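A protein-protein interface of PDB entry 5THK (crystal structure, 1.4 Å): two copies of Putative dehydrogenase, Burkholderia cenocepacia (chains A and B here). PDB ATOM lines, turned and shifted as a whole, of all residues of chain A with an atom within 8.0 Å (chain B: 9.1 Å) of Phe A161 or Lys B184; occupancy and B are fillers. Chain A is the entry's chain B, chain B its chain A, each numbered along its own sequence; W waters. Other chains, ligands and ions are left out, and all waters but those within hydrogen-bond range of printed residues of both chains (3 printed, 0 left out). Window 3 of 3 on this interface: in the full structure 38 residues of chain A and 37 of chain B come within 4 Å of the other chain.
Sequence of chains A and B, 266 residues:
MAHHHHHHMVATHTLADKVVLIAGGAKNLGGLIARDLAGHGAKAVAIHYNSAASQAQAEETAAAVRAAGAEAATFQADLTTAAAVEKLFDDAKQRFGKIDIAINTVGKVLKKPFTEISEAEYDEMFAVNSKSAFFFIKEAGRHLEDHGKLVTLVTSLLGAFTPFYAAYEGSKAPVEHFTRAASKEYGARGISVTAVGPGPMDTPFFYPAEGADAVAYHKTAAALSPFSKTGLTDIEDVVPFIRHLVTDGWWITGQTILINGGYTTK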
ATOM      1  N   SER A 156     -36.838   5.576  16.178  1.00  0.00           N
ATOM      2  CA  SER A 156     -37.215   6.209  14.917  1.00  0.00           C
ATOM      3  C   SER A 156     -36.081   6.235  13.894  1.00  0.00           C
ATOM      4  O   SER A 156     -36.343   6.508  12.714  1.00  0.00           O
ATOM      5  CB  SER A 156     -37.748   7.630  15.152  1.00  0.00           C
ATOM      6  OG  SER A 156     -39.128   7.597  15.490  1.00  0.00           O
ATOM      7  N   LEU A 157     -34.833   5.970  14.305  1.00  0.00           N
ATOM      8  CA  LEU A 157     -33.768   5.830  13.320  1.00  0.00           C
ATOM      9  C   LEU A 157     -33.992   4.669  12.358  1.00  0.00           C
ATOM     10  O   LEU A 157     -33.334   4.625  11.311  1.00  0.00           O
ATOM     11  CB  LEU A 157     -32.406   5.711  14.008  1.00  0.00           C
ATOM     12  CG  LEU A 157     -32.023   6.975  14.776  1.00  0.00           C
ATOM     13  CD1 LEU A 157     -30.789   6.716  15.641  1.00  0.00           C
ATOM     14  CD2 LEU A 157     -31.787   8.167  13.841  1.00  0.00           C
ATOM     15  N   LEU A 158     -34.915   3.749  12.656  1.00  0.00           N
ATOM     16  CA  LEU A 158     -35.282   2.741  11.661  1.00  0.00           C
ATOM     17  C   LEU A 158     -35.825   3.365  10.383  1.00  0.00           C
ATOM     18  O   LEU A 158     -35.794   2.715   9.332  1.00  0.00           O
ATOM     19  CB  LEU A 158     -36.266   1.724  12.238  1.00  0.00           C
ATOM     20  CG  LEU A 158     -35.701   0.831  13.345  1.00  0.00           C
ATOM     21  CD1 LEU A 158     -36.773  -0.115  13.859  1.00  0.00           C
ATOM     22  CD2 LEU A 158     -34.461   0.059  12.860  1.00  0.00           C
ATOM     23  N   GLY A 159     -36.328   4.600  10.446  1.00  0.00           N
ATOM     24  CA  GLY A 159     -36.775   5.319   9.273  1.00  0.00           C
ATOM     25  C   GLY A 159     -35.784   6.328   8.739  1.00  0.00           C
ATOM     26  O   GLY A 159     -36.141   7.127   7.860  1.00  0.00           O
ATOM     27  N   ALA A 160     -34.547   6.319   9.230  1.00  0.00           N
ATOM     28  CA  ALA A 160     -33.553   7.305   8.851  1.00  0.00           C
ATOM     29  C   ALA A 160     -32.572   6.735   7.834  1.00  0.00           C
ATOM     30  O   ALA A 160     -32.435   5.514   7.669  1.00  0.00           O
ATOM     31  CB  ALA A 160     -32.777   7.785  10.075  1.00  0.00           C
ATOM     32  N   PHE A 161     -31.875   7.648   7.164  1.00  0.00           N
ATOM     33  CA  PHE A 161     -30.815   7.333   6.203  1.00  0.00           C
ATOM     34  C   PHE A 161     -29.651   8.237   6.602  1.00  0.00           C
ATOM     35  O   PHE A 161     -29.544   9.367   6.117  1.00  0.00           O
ATOM     36  CB  PHE A 161     -31.293   7.614   4.777  1.00  0.00           C
ATOM     37  CG  PHE A 161     -30.338   7.158   3.692  1.00  0.00           C
ATOM     38  CD1 PHE A 161     -29.269   6.309   3.963  1.00  0.00           C
ATOM     39  CD2 PHE A 161     -30.523   7.596   2.391  1.00  0.00           C
ATOM     40  CE1 PHE A 161     -28.405   5.903   2.943  1.00  0.00           C
ATOM     41  CE2 PHE A 161     -29.664   7.201   1.371  1.00  0.00           C
ATOM     42  CZ  PHE A 161     -28.606   6.348   1.640  1.00  0.00           C
ATOM     43  N   THR A 162     -28.791   7.750   7.496  1.00  0.00           N
ATOM     44  CA  THR A 162     -27.892   8.658   8.195  1.00  0.00           C
ATOM     45  C   THR A 162     -26.652   7.894   8.661  1.00  0.00           C
ATOM     46  O   THR A 162     -26.721   6.679   8.884  1.00  0.00           O
ATOM     47  CB  THR A 162     -28.657   9.289   9.380  1.00  0.00           C
ATOM     48  OG1 THR A 162     -28.061  10.534   9.778  1.00  0.00           O
ATOM     49  CG2 THR A 162     -28.776   8.305  10.568  1.00  0.00           C
ATOM     50  N   PRO A 163     -25.512   8.564   8.805  1.00  0.00           N
ATOM     51  CA  PRO A 163     -24.308   7.888   9.304  1.00  0.00           C
ATOM     52  C   PRO A 163     -24.325   7.744  10.821  1.00  0.00           C
ATOM     53  O   PRO A 163     -25.129   8.350  11.530  1.00  0.00           O
ATOM     54  CB  PRO A 163     -23.182   8.846   8.895  1.00  0.00           C
ATOM     55  CG  PRO A 163     -23.852  10.222   8.941  1.00  0.00           C
ATOM     56  CD  PRO A 163     -25.233   9.942   8.369  1.00  0.00           C
ATOM     57  N   PHE A 164     -23.420   6.893  11.312  1.00  0.00           N
ATOM     58  CA  PHE A 164     -22.926   6.835  12.690  1.00  0.00           C
ATOM     59  C   PHE A 164     -23.750   5.970  13.640  1.00  0.00           C
ATOM     60  O   PHE A 164     -23.316   5.742  14.770  1.00  0.00           O
ATOM     61  CB  PHE A 164     -22.702   8.221  13.326  1.00  0.00           C
ATOM     62  CG  PHE A 164     -21.837   9.134  12.504  1.00  0.00           C
ATOM     63  CD1 PHE A 164     -20.633   8.687  11.980  1.00  0.00           C
ATOM     64  CD2 PHE A 164     -22.238  10.429  12.229  1.00  0.00           C
ATOM     65  CE1 PHE A 164     -19.830   9.521  11.216  1.00  0.00           C
ATOM     66  CE2 PHE A 164     -21.440  11.268  11.458  1.00  0.00           C
ATOM     67  CZ  PHE A 164     -20.237  10.815  10.952  1.00  0.00           C
ATOM     68  N   TYR A 165     -24.926   5.493  13.240  1.00  0.00           N
ATOM     69  CA  TYR A 165     -25.735   4.679  14.135  1.00  0.00           C
ATOM     70  C   TYR A 165     -25.787   3.207  13.731  1.00  0.00           C
ATOM     71  O   TYR A 165     -26.716   2.503  14.124  1.00  0.00           O
ATOM     72  CB  TYR A 165     -27.149   5.249  14.262  1.00  0.00           C
ATOM     73  CG  TYR A 165     -27.265   6.625  14.905  1.00  0.00           C
ATOM     74  CD1 TYR A 165     -27.211   6.790  16.291  1.00  0.00           C
ATOM     75  CD2 TYR A 165     -27.467   7.754  14.121  1.00  0.00           C
ATOM     76  CE1 TYR A 165     -27.356   8.057  16.876  1.00  0.00           C
ATOM     77  CE2 TYR A 165     -27.610   9.011  14.691  1.00  0.00           C
ATOM     78  CZ  TYR A 165     -27.553   9.156  16.062  1.00  0.00           C
ATOM     79  OH  TYR A 165     -27.694  10.422  16.603  1.00  0.00           O
ATOM     80  N   GLU A 169     -29.102   1.597  15.283  1.00  0.00           N
ATOM     81  CA  GLU A 169     -30.141   1.317  14.299  1.00  0.00           C
ATOM     82  C   GLU A 169     -30.099  -0.149  13.865  1.00  0.00           C
ATOM     83  O   GLU A 169     -31.144  -0.810  13.753  1.00  0.00           O
ATOM     84  CB  GLU A 169     -29.915   2.255  13.111  1.00  0.00           C
ATOM     85  CG  GLU A 169     -30.943   2.211  12.011  1.00  0.00           C
ATOM     86  CD  GLU A 169     -30.517   3.039  10.817  1.00  0.00           C
ATOM     87  OE1 GLU A 169     -29.699   3.971  10.991  1.00  0.00           O
ATOM     88  OE2 GLU A 169     -30.992   2.752   9.695  1.00  0.00           O
ATOM     89  N   THR A 264     -38.888  11.133  11.466  1.00  0.00           N
ATOM     90  CA  THR A 264     -38.754  10.198  10.357  1.00  0.00           C
ATOM     91  C   THR A 264     -40.119   9.566  10.093  1.00  0.00           C
ATOM     92  O   THR A 264     -41.051   9.671  10.901  1.00  0.00           O
ATOM     93  CB  THR A 264     -37.743   9.087  10.680  1.00  0.00           C
ATOM     94  OG1 THR A 264     -38.106   8.482  11.929  1.00  0.00           O
ATOM     95  CG2 THR A 264     -36.335   9.640  10.770  1.00  0.00           C
ATOM     96  N   GLU B 176     -29.527  -4.378   6.323  1.00  0.00           N
ATOM     97  CA  GLU B 176     -30.125  -3.251   5.609  1.00  0.00           C
ATOM     98  C   GLU B 176     -29.698  -1.932   6.236  1.00  0.00           C
ATOM     99  O   GLU B 176     -29.393  -0.957   5.533  1.00  0.00           O
ATOM    100  CB  GLU B 176     -31.651  -3.378   5.616  1.00  0.00           C
ATOM    101  CG  GLU B 176     -32.349  -2.097   5.176  1.00  0.00           C
ATOM    102  CD  GLU B 176     -33.814  -2.282   4.842  1.00  0.00           C
ATOM    103  OE1 GLU B 176     -34.379  -3.355   5.159  1.00  0.00           O
ATOM    104  OE2 GLU B 176     -34.401  -1.347   4.252  1.00  0.00           O
ATOM    105  N   HIS B 177     -29.654  -1.893   7.564  1.00  0.00           N
ATOM    106  CA  HIS B 177     -29.302  -0.669   8.264  1.00  0.00           C
ATOM    107  C   HIS B 177     -27.793  -0.440   8.286  1.00  0.00           C
ATOM    108  O   HIS B 177     -27.347   0.708   8.168  1.00  0.00           O
ATOM    109  CB  HIS B 177     -29.979  -0.654   9.638  1.00  0.00           C
ATOM    110  CG  HIS B 177     -31.471  -0.665   9.524  1.00  0.00           C
ATOM    111  ND1 HIS B 177     -32.216   0.491   9.430  1.00  0.00           N
ATOM    112  CD2 HIS B 177     -32.340  -1.690   9.360  1.00  0.00           C
ATOM    113  CE1 HIS B 177     -33.490   0.176   9.268  1.00  0.00           C
ATOM    114  NE2 HIS B 177     -33.590  -1.141   9.217  1.00  0.00           N
ATOM    115  N   PHE B 178     -26.989  -1.508   8.391  1.00  0.00           N
ATOM    116  CA  PHE B 178     -25.549  -1.347   8.189  1.00  0.00           C
ATOM    117  C   PHE B 178     -25.271  -0.740   6.817  1.00  0.00           C
ATOM    118  O   PHE B 178     -24.368   0.089   6.661  1.00  0.00           O
ATOM    119  CB  PHE B 178     -24.820  -2.693   8.239  1.00  0.00           C
ATOM    120  CG  PHE B 178     -24.979  -3.483   9.520  1.00  0.00           C
ATOM    121  CD1 PHE B 178     -25.351  -2.895  10.729  1.00  0.00           C
ATOM    122  CD2 PHE B 178     -24.710  -4.849   9.498  1.00  0.00           C
ATOM    123  CE1 PHE B 178     -25.481  -3.673  11.882  1.00  0.00           C
ATOM    124  CE2 PHE B 178     -24.830  -5.625  10.647  1.00  0.00           C
ATOM    125  CZ  PHE B 178     -25.216  -5.036  11.833  1.00  0.00           C
ATOM    126  N   THR B 179     -26.033  -1.165   5.804  1.00  0.00           N
ATOM    127  CA  THR B 179     -25.824  -0.701   4.436  1.00  0.00           C
ATOM    128  C   THR B 179     -26.168   0.783   4.296  1.00  0.00           C
ATOM    129  O   THR B 179     -25.462   1.525   3.603  1.00  0.00           O
ATOM    130  CB  THR B 179     -26.649  -1.602   3.500  1.00  0.00           C
ATOM    131  OG1 THR B 179     -26.095  -2.932   3.521  1.00  0.00           O
ATOM    132  CG2 THR B 179     -26.680  -1.090   2.076  1.00  0.00           C
ATOM    133  N   ARG B 180     -27.230   1.240   4.970  1.00  0.00           N
ATOM    134  CA  ARG B 180     -27.553   2.666   4.994  1.00  0.00           C
ATOM    135  C   ARG B 180     -26.412   3.482   5.581  1.00  0.00           C
ATOM    136  O   ARG B 180     -25.956   4.457   4.972  1.00  0.00           O
ATOM    137  CB  ARG B 180     -28.824   2.902   5.811  1.00  0.00           C
ATOM    138  CG  ARG B 180     -30.085   2.322   5.218  1.00  0.00           C
ATOM    139  CD  ARG B 180     -31.314   2.811   5.993  1.00  0.00           C
ATOM    140  NE  ARG B 180     -32.504   2.033   5.636  1.00  0.00           N
ATOM    141  CZ  ARG B 180     -33.700   2.170   6.207  1.00  0.00           C
ATOM    142  NH1 ARG B 180     -33.896   3.075   7.155  1.00  0.00           N
ATOM    143  NH2 ARG B 180     -34.701   1.397   5.813  1.00  0.00           N
ATOM    144  N   ALA B 181     -25.947   3.105   6.778  1.00  0.00           N
ATOM    145  CA  ALA B 181     -24.906   3.877   7.452  1.00  0.00           C
ATOM    146  C   ALA B 181     -23.608   3.868   6.651  1.00  0.00           C
ATOM    147  O   ALA B 181     -22.956   4.911   6.486  1.00  0.00           O
ATOM    148  CB  ALA B 181     -24.678   3.310   8.854  1.00  0.00           C
ATOM    149  N   ALA B 182     -23.203   2.691   6.162  1.00  0.00           N
ATOM    150  CA  ALA B 182     -21.953   2.594   5.407  1.00  0.00           C
ATOM    151  C   ALA B 182     -22.033   3.351   4.086  1.00  0.00           C
ATOM    152  O   ALA B 182     -21.038   3.933   3.636  1.00  0.00           O
ATOM    153  CB  ALA B 182     -21.605   1.126   5.162  1.00  0.00           C
ATOM    154  N   SER B 183     -23.198   3.356   3.435  1.00  0.00           N
ATOM    155  CA  SER B 183     -23.351   4.144   2.212  1.00  0.00           C
ATOM    156  C   SER B 183     -23.041   5.612   2.468  1.00  0.00           C
ATOM    157  O   SER B 183     -22.340   6.265   1.681  1.00  0.00           O
ATOM    158  CB  SER B 183     -24.779   3.983   1.691  1.00  0.00           C
ATOM    159  OG  SER B 183     -25.074   4.868   0.622  1.00  0.00           O
ATOM    160  N   LYS B 184     -23.558   6.147   3.580  1.00  0.00           N
ATOM    161  CA  LYS B 184     -23.319   7.545   3.925  1.00  0.00           C
ATOM    162  C   LYS B 184     -21.870   7.774   4.335  1.00  0.00           C
ATOM    163  O   LYS B 184     -21.264   8.782   3.953  1.00  0.00           O
ATOM    164  CB  LYS B 184     -24.259   7.976   5.058  1.00  0.00           C
ATOM    165  CG  LYS B 184     -25.736   8.077   4.653  1.00  0.00           C
ATOM    166  CD  LYS B 184     -25.924   9.100   3.551  1.00  0.00           C
ATOM    167  CE  LYS B 184     -27.357   9.580   3.460  1.00  0.00           C
ATOM    168  NZ  LYS B 184     -27.507  10.611   2.390  1.00  0.00           N
ATOM    169  N   GLU B 185     -21.298   6.858   5.122  1.00  0.00           N
ATOM    170  CA  GLU B 185     -19.956   7.066   5.661  1.00  0.00           C
ATOM    171  C   GLU B 185     -18.865   6.813   4.631  1.00  0.00           C
ATOM    172  O   GLU B 185     -17.817   7.460   4.689  1.00  0.00           O
ATOM    173  CB  GLU B 185     -19.740   6.176   6.891  1.00  0.00           C
ATOM    174  CG  GLU B 185     -20.648   6.530   8.082  1.00  0.00           C
ATOM    175  CD  GLU B 185     -20.386   5.669   9.309  1.00  0.00           C
ATOM    176  OE1 GLU B 185     -19.209   5.344   9.574  1.00  0.00           O
ATOM    177  OE2 GLU B 185     -21.357   5.311  10.014  1.00  0.00           O
ATOM    178  N   TYR B 186     -19.078   5.878   3.704  1.00  0.00           N
ATOM    179  CA  TYR B 186     -18.063   5.516   2.722  1.00  0.00           C
ATOM    180  C   TYR B 186     -18.233   6.247   1.395  1.00  0.00           C
ATOM    181  O   TYR B 186     -17.338   6.177   0.546  1.00  0.00           O
ATOM    182  CB  TYR B 186     -18.072   4.000   2.452  1.00  0.00           C
ATOM    183  CG  TYR B 186     -17.851   3.083   3.652  1.00  0.00           C
ATOM    184  CD1 TYR B 186     -17.452   3.581   4.893  1.00  0.00           C
ATOM    185  CD2 TYR B 186     -18.043   1.709   3.533  1.00  0.00           C
ATOM    186  CE1 TYR B 186     -17.247   2.735   5.982  1.00  0.00           C
ATOM    187  CE2 TYR B 186     -17.844   0.852   4.615  1.00  0.00           C
ATOM    188  CZ  TYR B 186     -17.454   1.375   5.843  1.00  0.00           C
ATOM    189  OH  TYR B 186     -17.246   0.543   6.927  1.00  0.00           O
ATOM    190  N   GLY B 187     -19.346   6.962   1.202  1.00  0.00           N
ATOM    191  CA  GLY B 187     -19.557   7.654  -0.059  1.00  0.00           C
ATOM    192  C   GLY B 187     -18.533   8.736  -0.344  1.00  0.00           C
ATOM    193  O   GLY B 187     -18.248   9.029  -1.508  1.00  0.00           O
ATOM    194  N   ALA B 188     -17.968   9.351   0.701  1.00  0.00           N
ATOM    195  CA  ALA B 188     -16.953  10.376   0.476  1.00  0.00           C
ATOM    196  C   ALA B 188     -15.721   9.830  -0.237  1.00  0.00           C
ATOM    197  O   ALA B 188     -14.988  10.610  -0.864  1.00  0.00           O
ATOM    198  CB  ALA B 188     -16.535  11.035   1.793  1.00  0.00           C
ATOM    199  N   ARG B 189     -15.478   8.519  -0.157  1.00  0.00           N
ATOM    200  CA  ARG B 189     -14.390   7.856  -0.871  1.00  0.00           C
ATOM    201  C   ARG B 189     -14.852   7.251  -2.189  1.00  0.00           C
ATOM    202  O   ARG B 189     -14.075   6.537  -2.835  1.00  0.00           O
ATOM    203  CB  ARG B 189     -13.769   6.731  -0.021  1.00  0.00           C
ATOM    204  CG  ARG B 189     -13.194   7.146   1.316  1.00  0.00           C
ATOM    205  CD  ARG B 189     -11.985   6.302   1.721  1.00  0.00           C
ATOM    206  NE  ARG B 189     -12.256   4.921   2.141  1.00  0.00           N
ATOM    207  CZ  ARG B 189     -11.822   3.841   1.494  1.00  0.00           C
ATOM    208  NH1 ARG B 189     -11.120   3.967   0.369  1.00  0.00           N
ATOM    209  NH2 ARG B 189     -12.085   2.628   1.972  1.00  0.00           N
ATOM    210  N   GLY B 190     -16.104   7.477  -2.582  1.00  0.00           N
ATOM    211  CA  GLY B 190     -16.599   6.964  -3.841  1.00  0.00           C
ATOM    212  C   GLY B 190     -17.094   5.533  -3.804  1.00  0.00           C
ATOM    213  O   GLY B 190     -17.338   4.950  -4.867  1.00  0.00           O
ATOM    214  N   ILE B 191     -17.252   4.953  -2.618  1.00  0.00           N
ATOM    215  CA  ILE B 191     -17.617   3.547  -2.471  1.00  0.00           C
ATOM    216  C   ILE B 191     -19.138   3.420  -2.483  1.00  0.00           C
ATOM    217  O   ILE B 191     -19.837   4.167  -1.780  1.00  0.00           O
ATOM    218  CB  ILE B 191     -17.017   2.976  -1.176  1.00  0.00           C
ATOM    219  CG1 ILE B 191     -15.486   2.927  -1.286  1.00  0.00           C
ATOM    220  CG2 ILE B 191     -17.614   1.582  -0.855  1.00  0.00           C
ATOM    221  CD1 ILE B 191     -14.802   2.702   0.039  1.00  0.00           C
ATOM    222  N   SER B 192     -19.652   2.474  -3.277  1.00  0.00           N
ATOM    223  CA  SER B 192     -21.079   2.156  -3.349  1.00  0.00           C
ATOM    224  C   SER B 192     -21.358   0.933  -2.490  1.00  0.00           C
ATOM    225  O   SER B 192     -20.653  -0.077  -2.613  1.00  0.00           O
ATOM    226  CB  SER B 192     -21.495   1.860  -4.791  1.00  0.00           C
ATOM    227  OG  SER B 192     -21.150   2.938  -5.649  1.00  0.00           O
ATOM    228  N   VAL B 193     -22.394   1.013  -1.643  1.00  0.00           N
ATOM    229  CA  VAL B 193     -22.715  -0.022  -0.660  1.00  0.00           C
ATOM    230  C   VAL B 193     -24.163  -0.449  -0.861  1.00  0.00           C
ATOM    231  O   VAL B 193     -25.069   0.390  -0.791  1.00  0.00           O
ATOM    232  CB  VAL B 193     -22.512   0.470   0.784  1.00  0.00           C
ATOM    233  CG1 VAL B 193     -22.672  -0.698   1.743  1.00  0.00           C
ATOM    234  CG2 VAL B 193     -21.147   1.140   0.955  1.00  0.00           C
ATOM    235  N   TRP B 251     -24.130   4.015  -9.214  1.00  0.00           N
ATOM    236  CA  TRP B 251     -24.922   5.079  -8.601  1.00  0.00           C
ATOM    237  C   TRP B 251     -25.977   4.539  -7.636  1.00  0.00           C
ATOM    238  O   TRP B 251     -26.509   5.317  -6.834  1.00  0.00           O
ATOM    239  CB  TRP B 251     -25.508   5.977  -9.704  1.00  0.00           C
ATOM    240  CG  TRP B 251     -26.058   7.320  -9.271  1.00  0.00           C
ATOM    241  CD1 TRP B 251     -27.361   7.737  -9.364  1.00  0.00           C
ATOM    242  CD2 TRP B 251     -25.325   8.423  -8.711  1.00  0.00           C
ATOM    243  NE1 TRP B 251     -27.478   9.030  -8.906  1.00  0.00           N
ATOM    244  CE2 TRP B 251     -26.251   9.465  -8.480  1.00  0.00           C
ATOM    245  CE3 TRP B 251     -23.978   8.631  -8.378  1.00  0.00           C
ATOM    246  CZ2 TRP B 251     -25.874  10.699  -7.938  1.00  0.00           C
ATOM    247  CZ3 TRP B 251     -23.605   9.856  -7.839  1.00  0.00           C
ATOM    248  CH2 TRP B 251     -24.546  10.870  -7.622  1.00  0.00           C
ATOM    249  N   ILE B 252     -26.267   3.236  -7.675  1.00  0.00           N
ATOM    250  CA  ILE B 252     -27.122   2.614  -6.667  1.00  0.00           C
ATOM    251  C   ILE B 252     -26.291   2.406  -5.406  1.00  0.00           C
ATOM    252  O   ILE B 252     -25.307   1.660  -5.411  1.00  0.00           O
ATOM    253  CB  ILE B 252     -27.713   1.286  -7.171  1.00  0.00           C
ATOM    254  CG1 ILE B 252     -28.543   1.513  -8.431  1.00  0.00           C
ATOM    255  CG2 ILE B 252     -28.559   0.638  -6.073  1.00  0.00           C
ATOM    256  CD1 ILE B 252     -28.985   0.214  -9.095  1.00  0.00           C
ATOM    257  N   THR B 253     -26.680   3.068  -4.319  1.00  0.00           N
ATOM    258  CA  THR B 253     -25.982   2.921  -3.050  1.00  0.00           C
ATOM    259  C   THR B 253     -26.944   3.238  -1.908  1.00  0.00           C
ATOM    260  O   THR B 253     -27.841   4.080  -2.040  1.00  0.00           O
ATOM    261  CB  THR B 253     -24.713   3.786  -2.994  1.00  0.00           C
ATOM    262  OG1 THR B 253     -23.995   3.501  -1.792  1.00  0.00           O
ATOM    263  CG2 THR B 253     -25.044   5.263  -3.038  1.00  0.00           C
ATOM    264  N   GLY B 254     -26.753   2.554  -0.785  1.00  0.00           N
ATOM    265  CA  GLY B 254     -27.625   2.739   0.358  1.00  0.00           C
ATOM    266  C   GLY B 254     -28.981   2.096   0.213  1.00  0.00           C
ATOM    267  O   GLY B 254     -29.925   2.511   0.898  1.00  0.00           O
ATOM    268  N   GLN B 255     -29.104   1.094  -0.653  1.00  0.00           N
ATOM    269  CA  GLN B 255     -30.359   0.430  -0.950  1.00  0.00           C
ATOM    270  C   GLN B 255     -30.246  -1.061  -0.658  1.00  0.00           C
ATOM    271  O   GLN B 255     -29.178  -1.670  -0.808  1.00  0.00           O
ATOM    272  CB  GLN B 255     -30.734   0.588  -2.435  1.00  0.00           C
ATOM    273  CG  GLN B 255     -30.596   2.008  -2.980  1.00  0.00           C
ATOM    274  CD  GLN B 255     -31.480   3.005  -2.255  1.00  0.00           C
ATOM    275  OE1 GLN B 255     -32.663   2.750  -2.023  1.00  0.00           O
ATOM    276  NE2 GLN B 255     -30.911   4.156  -1.909  1.00  0.00           N
ATOM    277  N   THR B 256     -31.369  -1.636  -0.247  1.00  0.00           N
ATOM    278  CA  THR B 256     -31.550  -3.077  -0.118  1.00  0.00           C
ATOM    279  C   THR B 256     -32.624  -3.464  -1.127  1.00  0.00           C
ATOM    280  O   THR B 256     -33.768  -3.010  -1.021  1.00  0.00           O
ATOM    281  CB  THR B 256     -31.966  -3.434   1.315  1.00  0.00           C
ATOM    282  OG1 THR B 256     -30.874  -3.160   2.206  1.00  0.00           O
ATOM    283  CG2 THR B 256     -32.351  -4.909   1.434  1.00  0.00           C
HETATM  284  O   HOH W   1     -37.365   2.500   6.304  1.00  0.00           O
HETATM  285  O   HOH W   2     -27.611   2.136  10.744  1.00  0.00           O
HETATM  286  O   HOH W   3     -22.019   3.760  12.244  1.00  0.00           O
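No position is printed for both chains. Of the 13 pairs that touch across the chains among the printed residues, none has its exchanged pair printed and touching as well.
Hydrophobic or aromatic side chains of chain B that line the printed part of chain A: His B177 and Ala B181.
OE2 of Glu A169 lies within salt-bridge range of NH1 of Arg B180 (3.9 Å). O of Ala A160 sits at hydrogen-bond distance from NH1 of Arg B180 (2.9 Å). The guanidinium group of Arg B180 lies within hydrogen-bond range of the backbone carbonyl oxygen of Leu A158 (2.9 Å). The backbone NH (N) of Phe A164 lies within hydrogen-bond range of the side-chain carboxylate (OE2) of Glu B185 (2.9 Å). ND1 of His B177 is in hydrogen-bond range of OE2 of Glu A169.
Water W2 bridges the side-chain carboxylate (OE1) of Glu A169 (2.8 Å) and the backbone carbonyl oxygen (O) of His B177 (3.0 Å). Water W3 lies within hydrogen-bond range of the side-chain carboxylate (OE2) of Glu B185 and the backbone carbonyl oxygen (O) of Phe A164. Water W1 bridges the guanidinium group (NH2) of Arg B180 (2.9 Å) and the backbone carbonyl oxygen (O) of Leu A158 (3.4 Å).
Among the printed residues, merely in contact across the chains: Leu A158 with His B177 (3.4 Å), Phe A161 with Lys B184 (3.4 Å), Phe A161 with Arg B180 (3.5 Å), Pro A163 with Glu B185 (3.5 Å), Thr A162 with Ala B181 (3.6 Å), Phe A161 with Gly B254 (3.95 Å), Phe A161 with Ser B183 (3.96 Å) and Pro A163 with Lys B184 (3.97 Å).
The backbone carbonyl oxygen of Val B193 lies within hydrogen-bond range of the backbone NH of Gly B254 (2.7 Å). The side-chain hydroxyl (OG) of Ser B183 is in hydrogen-bond range of the backbone NH (N) of Gly B254 (3.2 Å). NH2 of Arg B180 is in salt-bridge range of OE2 of Glu B176. OG of Ser B183 lies within hydrogen-bond range of OG1 of Thr B253 (3.0 Å).
Printed residues of chain B within 4 Å of Phe A161: Arg B180 (3.5 Å), Ser B183 (3.96 Å), Lys B184 (3.4 Å) and Gly B254 (3.95 Å). Lys B184 touches just these residues of chain A: Phe A161 and Pro A163. Of chain B, only Arg B180 (2.9 Å) comes within 4 Å of Ala A160. Printed residues of chain B within 4 Å of Phe A164: Glu B185. Printed residues of chain A within 4 Å of Ser B183: Phe A161 (3.96 Å). Gln B255 touches none of the printed residues of chain A. Gly A159 touches none of the printed residues of chain B. The nearest printed residue of chain B that does not touch Phe A161 is Thr B253 (4.4 Å). The nearest residue of chain A that does not touch Lys B184 is Thr A162 (4.1 Å). The nearest printed residue of chain A that does not touch His B177 is Leu A157 (4.7 Å).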
